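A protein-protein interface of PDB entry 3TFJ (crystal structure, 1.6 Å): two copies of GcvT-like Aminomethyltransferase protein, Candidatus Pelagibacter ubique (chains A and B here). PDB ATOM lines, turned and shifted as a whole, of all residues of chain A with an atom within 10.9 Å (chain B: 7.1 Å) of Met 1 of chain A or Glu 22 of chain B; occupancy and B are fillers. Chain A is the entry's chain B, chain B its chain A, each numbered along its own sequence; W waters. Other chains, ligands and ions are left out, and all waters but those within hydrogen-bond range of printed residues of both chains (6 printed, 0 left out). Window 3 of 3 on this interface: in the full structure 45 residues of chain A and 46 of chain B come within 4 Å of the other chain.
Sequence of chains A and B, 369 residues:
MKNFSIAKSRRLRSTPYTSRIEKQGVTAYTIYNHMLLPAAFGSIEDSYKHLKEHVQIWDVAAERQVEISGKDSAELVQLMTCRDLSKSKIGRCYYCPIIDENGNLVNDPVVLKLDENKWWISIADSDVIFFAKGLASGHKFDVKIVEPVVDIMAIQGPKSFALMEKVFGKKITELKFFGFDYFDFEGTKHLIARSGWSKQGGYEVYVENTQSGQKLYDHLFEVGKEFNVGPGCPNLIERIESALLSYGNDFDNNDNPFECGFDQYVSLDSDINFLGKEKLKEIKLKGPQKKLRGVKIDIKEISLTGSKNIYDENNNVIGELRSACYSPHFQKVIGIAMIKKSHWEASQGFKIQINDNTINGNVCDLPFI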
ATOM      1  N   MET A   1      17.566  -7.976 -18.351  1.00  0.00           N
ATOM      2  CA  MET A   1      16.198  -8.220 -17.804  1.00  0.00           C
ATOM      3  C   MET A   1      15.085  -7.530 -18.615  1.00  0.00           C
ATOM      4  O   MET A   1      14.875  -6.308 -18.577  1.00  0.00           O
ATOM      5  CB  MET A   1      16.106  -7.920 -16.271  1.00  0.00           C
ATOM      6  CG  MET A   1      14.675  -7.520 -15.689  1.00  0.00           C
ATOM      7  SD  MET A   1      13.457  -8.769 -15.090  1.00  0.00           S
ATOM      8  CE  MET A   1      12.100  -7.627 -14.766  1.00  0.00           C
ATOM      9  N   LYS A   2      14.429  -8.373 -19.435  1.00  0.00           N
ATOM     10  CA  LYS A   2      12.944  -8.315 -19.734  1.00  0.00           C
ATOM     11  C   LYS A   2      12.435  -9.754 -20.101  1.00  0.00           C
ATOM     12  O   LYS A   2      11.722 -10.295 -19.301  1.00  0.00           O
ATOM     13  CB  LYS A   2      12.434  -7.303 -20.716  1.00  0.00           C
ATOM     14  CG  LYS A   2      10.968  -6.969 -20.450  1.00  0.00           C
ATOM     15  CD  LYS A   2      10.009  -7.838 -21.238  1.00  0.00           C
ATOM     16  CE  LYS A   2       9.504  -7.172 -22.501  1.00  0.00           C
ATOM     17  NZ  LYS A   2       8.739  -8.140 -23.352  1.00  0.00           N
ATOM     18  N   ASN A   3      12.761 -10.309 -21.281  1.00  0.00           N
ATOM     19  CA  ASN A   3      12.638 -11.748 -21.502  1.00  0.00           C
ATOM     20  C   ASN A   3      14.010 -12.386 -21.287  1.00  0.00           C
ATOM     21  O   ASN A   3      15.058 -11.752 -21.374  1.00  0.00           O
ATOM     22  CB  ASN A   3      12.117 -12.149 -22.897  1.00  0.00           C
ATOM     23  CG  ASN A   3      10.649 -11.935 -23.036  1.00  0.00           C
ATOM     24  OD1 ASN A   3       9.873 -12.177 -22.097  1.00  0.00           O
ATOM     25  ND2 ASN A   3      10.259 -11.376 -24.157  1.00  0.00           N
ATOM     26  N   PHE A   4      13.980 -13.664 -20.969  1.00  0.00           N
ATOM     27  CA  PHE A   4      15.126 -14.532 -20.719  1.00  0.00           C
ATOM     28  C   PHE A   4      15.007 -15.769 -21.553  1.00  0.00           C
ATOM     29  O   PHE A   4      13.894 -16.341 -21.722  1.00  0.00           O
ATOM     30  CB  PHE A   4      15.210 -14.927 -19.218  1.00  0.00           C
ATOM     31  CG  PHE A   4      15.223 -13.707 -18.296  1.00  0.00           C
ATOM     32  CD1 PHE A   4      16.412 -13.027 -18.034  1.00  0.00           C
ATOM     33  CD2 PHE A   4      14.041 -13.175 -17.798  1.00  0.00           C
ATOM     34  CE1 PHE A   4      16.416 -11.947 -17.257  1.00  0.00           C
ATOM     35  CE2 PHE A   4      14.084 -12.054 -17.022  1.00  0.00           C
ATOM     36  CZ  PHE A   4      15.267 -11.453 -16.777  1.00  0.00           C
ATOM     37  N   SER A   5      16.156 -16.260 -22.002  1.00  0.00           N
ATOM     38  CA  SER A   5      16.186 -17.461 -22.835  1.00  0.00           C
ATOM     39  C   SER A   5      16.064 -18.693 -22.006  1.00  0.00           C
ATOM     40  O   SER A   5      16.521 -18.739 -20.866  1.00  0.00           O
ATOM     41  CB  SER A   5      17.461 -17.554 -23.670  1.00  0.00           C
ATOM     42  OG  SER A   5      17.555 -16.452 -24.543  1.00  0.00           O
ATOM     43  N   SER A 303       1.577  -8.879 -16.367  1.00  0.00           N
ATOM     44  CA  SER A 303       2.534  -9.976 -16.624  1.00  0.00           C
ATOM     45  C   SER A 303       2.743 -10.702 -15.323  1.00  0.00           C
ATOM     46  O   SER A 303       3.722 -10.434 -14.575  1.00  0.00           O
ATOM     47  CB  SER A 303       3.879  -9.482 -17.161  1.00  0.00           C
ATOM     48  OG  SER A 303       4.777 -10.581 -17.293  1.00  0.00           O
ATOM     49  N   LEU A 304       1.815 -11.622 -15.031  1.00  0.00           N
ATOM     50  CA  LEU A 304       1.797 -12.274 -13.738  1.00  0.00           C
ATOM     51  C   LEU A 304       2.815 -13.433 -13.633  1.00  0.00           C
ATOM     52  O   LEU A 304       2.808 -14.368 -14.482  1.00  0.00           O
ATOM     53  CB  LEU A 304       0.375 -12.703 -13.425  1.00  0.00           C
ATOM     54  CG  LEU A 304       0.186 -13.127 -11.982  1.00  0.00           C
ATOM     55  CD1 LEU A 304       0.130 -11.841 -11.080  1.00  0.00           C
ATOM     56  CD2 LEU A 304      -1.084 -13.966 -11.863  1.00  0.00           C
ATOM     57  N   THR A 305       3.707 -13.400 -12.621  1.00  0.00           N
ATOM     58  CA  THR A 305       4.768 -14.418 -12.584  1.00  0.00           C
ATOM     59  C   THR A 305       4.712 -15.248 -11.313  1.00  0.00           C
ATOM     60  O   THR A 305       5.537 -16.135 -11.098  1.00  0.00           O
ATOM     61  CB  THR A 305       6.183 -13.749 -12.731  1.00  0.00           C
ATOM     62  OG1 THR A 305       6.430 -12.872 -11.626  1.00  0.00           O
ATOM     63  CG2 THR A 305       6.259 -12.989 -14.000  1.00  0.00           C
ATOM     64  N   GLY A 306       3.773 -14.920 -10.444  1.00  0.00           N
ATOM     65  CA  GLY A 306       3.662 -15.521  -9.133  1.00  0.00           C
ATOM     66  C   GLY A 306       2.453 -14.912  -8.464  1.00  0.00           C
ATOM     67  O   GLY A 306       1.815 -14.041  -9.055  1.00  0.00           O
ATOM     68  N   ASN A 355       2.700  -1.580  -9.716  1.00  0.00           N
ATOM     69  CA  ASN A 355       3.659  -0.491  -9.873  1.00  0.00           C
ATOM     70  C   ASN A 355       3.191   0.774  -9.140  1.00  0.00           C
ATOM     71  O   ASN A 355       2.867   0.656  -7.971  1.00  0.00           O
ATOM     72  CB  ASN A 355       3.978  -0.271 -11.369  1.00  0.00           C
ATOM     73  CG  ASN A 355       4.801  -1.397 -11.958  1.00  0.00           C
ATOM     74  OD1 ASN A 355       5.987  -1.556 -11.627  1.00  0.00           O
ATOM     75  ND2 ASN A 355       4.196  -2.170 -12.864  1.00  0.00           N
ATOM     76  N   LYS B   8       7.177 -17.194 -18.130  1.00  0.00           N
ATOM     77  CA  LYS B   8       7.004 -17.280 -16.682  1.00  0.00           C
ATOM     78  C   LYS B   8       5.519 -17.465 -16.325  1.00  0.00           C
ATOM     79  O   LYS B   8       4.624 -17.046 -17.073  1.00  0.00           O
ATOM     80  CB  LYS B   8       7.537 -16.036 -16.045  1.00  0.00           C
ATOM     81  CG  LYS B   8       9.092 -15.969 -16.061  1.00  0.00           C
ATOM     82  CD  LYS B   8       9.516 -14.908 -15.213  1.00  0.00           C
ATOM     83  CE  LYS B   8      11.006 -14.849 -15.219  1.00  0.00           C
ATOM     84  NZ  LYS B   8      11.262 -13.641 -14.358  1.00  0.00           N
ATOM     85  N   SER B  14       9.125 -18.665  -9.102  1.00  0.00           N
ATOM     86  CA  SER B  14      10.255 -17.770  -8.862  1.00  0.00           C
ATOM     87  C   SER B  14      10.784 -18.091  -7.442  1.00  0.00           C
ATOM     88  O   SER B  14      10.240 -18.964  -6.704  1.00  0.00           O
ATOM     89  CB  SER B  14       9.883 -16.301  -9.153  1.00  0.00           C
ATOM     90  OG  SER B  14       9.651 -16.021 -10.569  1.00  0.00           O
ATOM     91  N   TYR B  17      15.404 -15.065  -4.643  1.00  0.00           N
ATOM     92  CA  TYR B  17      16.526 -14.380  -5.236  1.00  0.00           C
ATOM     93  C   TYR B  17      16.255 -13.898  -6.684  1.00  0.00           C
ATOM     94  O   TYR B  17      17.105 -13.194  -7.260  1.00  0.00           O
ATOM     95  CB  TYR B  17      17.780 -15.251  -5.177  1.00  0.00           C
ATOM     96  CG  TYR B  17      17.953 -15.980  -3.876  1.00  0.00           C
ATOM     97  CD1 TYR B  17      18.242 -15.301  -2.710  1.00  0.00           C
ATOM     98  CD2 TYR B  17      17.715 -17.336  -3.756  1.00  0.00           C
ATOM     99  CE1 TYR B  17      18.355 -15.951  -1.517  1.00  0.00           C
ATOM    100  CE2 TYR B  17      17.847 -17.991  -2.562  1.00  0.00           C
ATOM    101  CZ  TYR B  17      18.152 -17.298  -1.424  1.00  0.00           C
ATOM    102  OH  TYR B  17      18.222 -17.907  -0.174  1.00  0.00           O
ATOM    103  N   THR B  18      15.090 -14.231  -7.247  1.00  0.00           N
ATOM    104  CA  THR B  18      14.828 -13.895  -8.632  1.00  0.00           C
ATOM    105  C   THR B  18      15.026 -12.414  -8.953  1.00  0.00           C
ATOM    106  O   THR B  18      15.675 -12.057  -9.939  1.00  0.00           O
ATOM    107  CB  THR B  18      13.398 -14.286  -8.982  1.00  0.00           C
ATOM    108  OG1 THR B  18      13.285 -15.716  -8.842  1.00  0.00           O
ATOM    109  CG2 THR B  18      13.029 -13.815 -10.427  1.00  0.00           C
ATOM    110  N   SER B  19      14.388 -11.529  -8.175  1.00  0.00           N
ATOM    111  CA  SER B  19      14.488 -10.132  -8.467  1.00  0.00           C
ATOM    112  C   SER B  19      15.900  -9.602  -8.399  1.00  0.00           C
ATOM    113  O   SER B  19      16.265  -8.723  -9.219  1.00  0.00           O
ATOM    114  CB  SER B  19      13.560  -9.283  -7.569  1.00  0.00           C
ATOM    115  OG  SER B  19      13.889  -9.284  -6.192  1.00  0.00           O
ATOM    116  N   ARG B  20      16.708 -10.183  -7.509  1.00  0.00           N
ATOM    117  CA  ARG B  20      18.114  -9.784  -7.440  1.00  0.00           C
ATOM    118  C   ARG B  20      18.882 -10.270  -8.669  1.00  0.00           C
ATOM    119  O   ARG B  20      19.640  -9.502  -9.277  1.00  0.00           O
ATOM    120  CB  ARG B  20      18.711 -10.342  -6.137  1.00  0.00           C
ATOM    121  CG  ARG B  20      18.217  -9.550  -4.914  1.00  0.00           C
ATOM    122  CD  ARG B  20      18.405 -10.391  -3.629  1.00  0.00           C
ATOM    123  NE  ARG B  20      18.239  -9.557  -2.441  1.00  0.00           N
ATOM    124  CZ  ARG B  20      17.092  -9.139  -1.929  1.00  0.00           C
ATOM    125  NH1 ARG B  20      15.910  -9.559  -2.351  1.00  0.00           N
ATOM    126  NH2 ARG B  20      17.130  -8.300  -0.896  1.00  0.00           N
ATOM    127  N   ILE B  21      18.783 -11.554  -8.969  1.00  0.00           N
ATOM    128  CA  ILE B  21      19.594 -12.068 -10.081  1.00  0.00           C
ATOM    129  C   ILE B  21      19.245 -11.440 -11.435  1.00  0.00           C
ATOM    130  O   ILE B  21      20.098 -11.307 -12.331  1.00  0.00           O
ATOM    131  CB  ILE B  21      19.652 -13.602 -10.154  1.00  0.00           C
ATOM    132  CG1 ILE B  21      18.294 -14.246 -10.562  1.00  0.00           C
ATOM    133  CG2 ILE B  21      20.206 -14.201  -8.823  1.00  0.00           C
ATOM    134  CD1 ILE B  21      18.374 -15.783 -10.738  1.00  0.00           C
ATOM    135  N   GLU B  22      18.004 -11.039 -11.563  1.00  0.00           N
ATOM    136  CA  GLU B  22      17.563 -10.338 -12.783  1.00  0.00           C
ATOM    137  C   GLU B  22      18.094  -8.924 -12.860  1.00  0.00           C
ATOM    138  O   GLU B  22      18.070  -8.339 -13.969  1.00  0.00           O
ATOM    139  CB  GLU B  22      16.042 -10.433 -12.982  1.00  0.00           C
ATOM    140  CG  GLU B  22      15.611 -11.851 -13.233  1.00  0.00           C
ATOM    141  CD  GLU B  22      14.144 -12.103 -13.505  1.00  0.00           C
ATOM    142  OE1 GLU B  22      13.327 -11.165 -13.545  1.00  0.00           O
ATOM    143  OE2 GLU B  22      13.837 -13.321 -13.770  1.00  0.00           O
ATOM    144  N   LYS B  23      18.538  -8.338 -11.755  1.00  0.00           N
ATOM    145  CA  LYS B  23      19.283  -7.087 -11.840  1.00  0.00           C
ATOM    146  C   LYS B  23      20.801  -7.299 -11.895  1.00  0.00           C
ATOM    147  O   LYS B  23      21.565  -6.361 -12.090  1.00  0.00           O
ATOM    148  CB  LYS B  23      18.851  -6.163 -10.705  1.00  0.00           C
ATOM    149  CG  LYS B  23      17.432  -5.604 -10.937  1.00  0.00           C
ATOM    150  CD  LYS B  23      16.762  -4.968  -9.673  1.00  0.00           C
ATOM    151  CE  LYS B  23      17.075  -5.785  -8.388  1.00  0.00           C
ATOM    152  NZ  LYS B  23      15.950  -6.058  -7.442  1.00  0.00           N
ATOM    153  N   GLN B  24      21.260  -8.536 -11.761  1.00  0.00           N
ATOM    154  CA  GLN B  24      22.679  -8.877 -11.762  1.00  0.00           C
ATOM    155  C   GLN B  24      23.118  -9.634 -13.012  1.00  0.00           C
ATOM    156  O   GLN B  24      24.212 -10.208 -13.085  1.00  0.00           O
ATOM    157  CB  GLN B  24      23.042  -9.680 -10.545  1.00  0.00           C
ATOM    158  CG  GLN B  24      22.927  -8.926  -9.258  1.00  0.00           C
ATOM    159  CD  GLN B  24      23.084  -9.820  -8.050  1.00  0.00           C
ATOM    160  OE1 GLN B  24      22.290 -10.717  -7.832  1.00  0.00           O
ATOM    161  NE2 GLN B  24      24.082  -9.515  -7.203  1.00  0.00           N
ATOM    162  N   GLY B  25      22.261  -9.663 -14.009  1.00  0.00           N
ATOM    163  CA  GLY B  25      22.720 -10.149 -15.285  1.00  0.00           C
ATOM    164  C   GLY B  25      22.383 -11.547 -15.731  1.00  0.00           C
ATOM    165  O   GLY B  25      23.036 -12.043 -16.636  1.00  0.00           O
ATOM    166  N   VAL B  26      21.422 -12.213 -15.102  1.00  0.00           N
ATOM    167  CA  VAL B  26      21.037 -13.539 -15.561  1.00  0.00           C
ATOM    168  C   VAL B  26      20.614 -13.404 -17.019  1.00  0.00           C
ATOM    169  O   VAL B  26      19.888 -12.467 -17.379  1.00  0.00           O
ATOM    170  CB  VAL B  26      19.993 -14.211 -14.677  1.00  0.00           C
ATOM    171  CG1 VAL B  26      18.611 -13.534 -14.725  1.00  0.00           C
ATOM    172  CG2 VAL B  26      19.932 -15.752 -14.907  1.00  0.00           C
ATOM    173  N   TYR B  29      17.679 -19.230 -18.249  1.00  0.00           N
ATOM    174  CA  TYR B  29      17.105 -20.076 -17.213  1.00  0.00           C
ATOM    175  C   TYR B  29      16.897 -21.513 -17.695  1.00  0.00           C
ATOM    176  O   TYR B  29      16.584 -21.774 -18.863  1.00  0.00           O
ATOM    177  CB  TYR B  29      15.732 -19.554 -16.728  1.00  0.00           C
ATOM    178  CG  TYR B  29      15.722 -18.362 -15.796  1.00  0.00           C
ATOM    179  CD1 TYR B  29      16.141 -18.492 -14.489  1.00  0.00           C
ATOM    180  CD2 TYR B  29      15.268 -17.125 -16.204  1.00  0.00           C
ATOM    181  CE1 TYR B  29      16.109 -17.406 -13.626  1.00  0.00           C
ATOM    182  CE2 TYR B  29      15.213 -16.069 -15.356  1.00  0.00           C
ATOM    183  CZ  TYR B  29      15.644 -16.200 -14.043  1.00  0.00           C
ATOM    184  OH  TYR B  29      15.524 -15.165 -13.138  1.00  0.00           O
ATOM    185  N   LEU B  36      12.406 -21.835 -11.339  1.00  0.00           N
ATOM    186  CA  LEU B  36      13.455 -21.179 -12.103  1.00  0.00           C
ATOM    187  C   LEU B  36      14.820 -21.426 -11.437  1.00  0.00           C
ATOM    188  O   LEU B  36      14.981 -21.185 -10.224  1.00  0.00           O
ATOM    189  CB  LEU B  36      13.188 -19.682 -12.153  1.00  0.00           C
ATOM    190  CG  LEU B  36      11.929 -19.298 -12.953  1.00  0.00           C
ATOM    191  CD1 LEU B  36      11.501 -17.847 -12.618  1.00  0.00           C
ATOM    192  CD2 LEU B  36      12.281 -19.407 -14.400  1.00  0.00           C
ATOM    193  N   PHE B  41      24.876 -16.532 -16.827  1.00  0.00           N
ATOM    194  CA  PHE B  41      25.078 -15.101 -16.624  1.00  0.00           C
ATOM    195  C   PHE B  41      26.108 -14.723 -17.706  1.00  0.00           C
ATOM    196  O   PHE B  41      27.292 -14.465 -17.442  1.00  0.00           O
ATOM    197  CB  PHE B  41      25.658 -14.764 -15.224  1.00  0.00           C
ATOM    198  CG  PHE B  41      24.691 -14.982 -14.083  1.00  0.00           C
ATOM    199  CD1 PHE B  41      24.439 -16.241 -13.608  1.00  0.00           C
ATOM    200  CD2 PHE B  41      23.986 -13.920 -13.551  1.00  0.00           C
ATOM    201  CE1 PHE B  41      23.468 -16.451 -12.613  1.00  0.00           C
ATOM    202  CE2 PHE B  41      23.090 -14.098 -12.514  1.00  0.00           C
ATOM    203  CZ  PHE B  41      22.812 -15.318 -12.059  1.00  0.00           C
ATOM    204  N   TYR B 217      22.320 -12.516   1.385  1.00  0.00           N
ATOM    205  CA  TYR B 217      22.675 -12.456  -0.027  1.00  0.00           C
ATOM    206  C   TYR B 217      23.265 -11.060  -0.342  1.00  0.00           C
ATOM    207  O   TYR B 217      24.369 -10.944  -0.906  1.00  0.00           O
ATOM    208  CB  TYR B 217      21.428 -12.787  -0.883  1.00  0.00           C
ATOM    209  CG  TYR B 217      21.662 -12.783  -2.365  1.00  0.00           C
ATOM    210  CD1 TYR B 217      21.677 -13.937  -3.067  1.00  0.00           C
ATOM    211  CD2 TYR B 217      21.811 -11.590  -3.070  1.00  0.00           C
ATOM    212  CE1 TYR B 217      21.848 -13.958  -4.421  1.00  0.00           C
ATOM    213  CE2 TYR B 217      22.006 -11.584  -4.459  1.00  0.00           C
ATOM    214  CZ  TYR B 217      22.018 -12.804  -5.130  1.00  0.00           C
ATOM    215  OH  TYR B 217      22.227 -12.871  -6.476  1.00  0.00           O
HETATM  216  O   HOH W   1      12.476  -9.611 -11.537  1.00  0.00           O
HETATM  217  O   HOH W   2       7.755 -17.171 -12.386  1.00  0.00           O
HETATM  218  O   HOH W   3       6.554 -17.607  -9.338  1.00  0.00           O
HETATM  219  O   HOH W   4      19.529 -10.682 -19.358  1.00  0.00           O
HETATM  220  O   HOH W   5       9.637 -13.314 -11.790  1.00  0.00           O
HETATM  221  O   HOH W   6      19.399  -9.923 -16.706  1.00  0.00           O
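O of Ser 5 of chain A sits at hydrogen-bond distance from N of Tyr 29 of chain B (2.9 Å).
SD of Met 1 of chain A sits close to OE1 of Glu 22 of chain B.
OE2 of Glu 22 of chain B is in salt-bridge range of NZ of Lys 8 of chain B (2.7 Å).
The backbone NH (N) of Val 26 of chain B lies within hydrogen-bond range of the backbone carbonyl oxygen (O) of Ile 21 of chain B, at 3.2 Å.
The side-chain carboxylate of Glu 22 of chain B is in hydrogen-bond range of the side-chain hydroxyl of Tyr 29 of chain B (2.6 Å).
Phe 4 of chain A touches Glu 22 of chain B (CE2 to OE2, 3.5 Å).
Val 26 of chain B touches Phe 4 of chain A (O to CE1, 3.5 Å).
Phe 4 of chain A touches Tyr 29 of chain B.
Thr 305 of chain A touches Lys 8 of chain B (CG2 to CB, 3.9 Å).
Of the printed residues of chain B, Met 1 of chain A touches Glu 22 (2.9 Å).
Printed residues of chain B within 4 Å of Phe 4 of chain A: Glu 22, Val 26 and Tyr 29.
Of the printed residues of chain B, Ser 5 of chain A touches Tyr 29 (2.9 Å).
Printed residues of chain B within 4 Å of Thr 305 of chain A: Lys 8 (3.9 Å).
Printed residues of chain A within 4 Å of Lys 8 of chain B: Thr 305.
No residue of chain A comes within 4 Å of Thr 18 of chain B.
No residue of chain A comes within 4 Å of Ile 21 of chain B.
Printed residues of chain A within 4 Å of Glu 22 of chain B: Met 1 and Phe 4.
No residue of chain A comes within 4 Å of Gly 25 of chain B.
Of chain A, only Phe 4 comes within 4 Å of Val 26 of chain B.
Of the printed residues of chain A, Tyr 29 of chain B touches Phe 4 and Ser 5.
The nearest printed residue of chain A that does not touch Glu 22 of chain B is Lys 2 of chain A (6.0 Å).
Of the 16 printed residues of chain B, 4 touch a printed residue of chain A.
No position is printed for both chains.
Water W3 lies within hydrogen-bond range of the backbone carbonyl oxygen (O) of Thr 305 of chain A and the backbone NH (N) of Ser 14 of chain B.
Water W6 lies within hydrogen-bond range of the backbone carbonyl oxygen (O) of Val 26 of chain B (2.7 Å), the backbone NH (N) of Met 1 of chain A (3.1 Å) and the backbone carbonyl oxygen (O) of Glu 22 of chain B (3.4 Å).
Water W1 bridges OE1 of Glu 22 of chain B (2.7 Å) and SD of Met 1 of chain A (3.8 Å).
Water W4 lies within hydrogen-bond range of the backbone carbonyl oxygen (O) of Val 26 of chain B (2.7 Å) and the backbone NH (N) of Met 1 of chain A (3.5 Å).
Water W2 bridges the backbone carbonyl oxygen of Thr 305 of chain A and the side-chain hydroxyl of Ser 14 of chain B.
Water W5 lies within hydrogen-bond range of OG of Ser 14 of chain B, NZ of Lys 8 of chain B and OG1 of Thr 305 of chain A.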
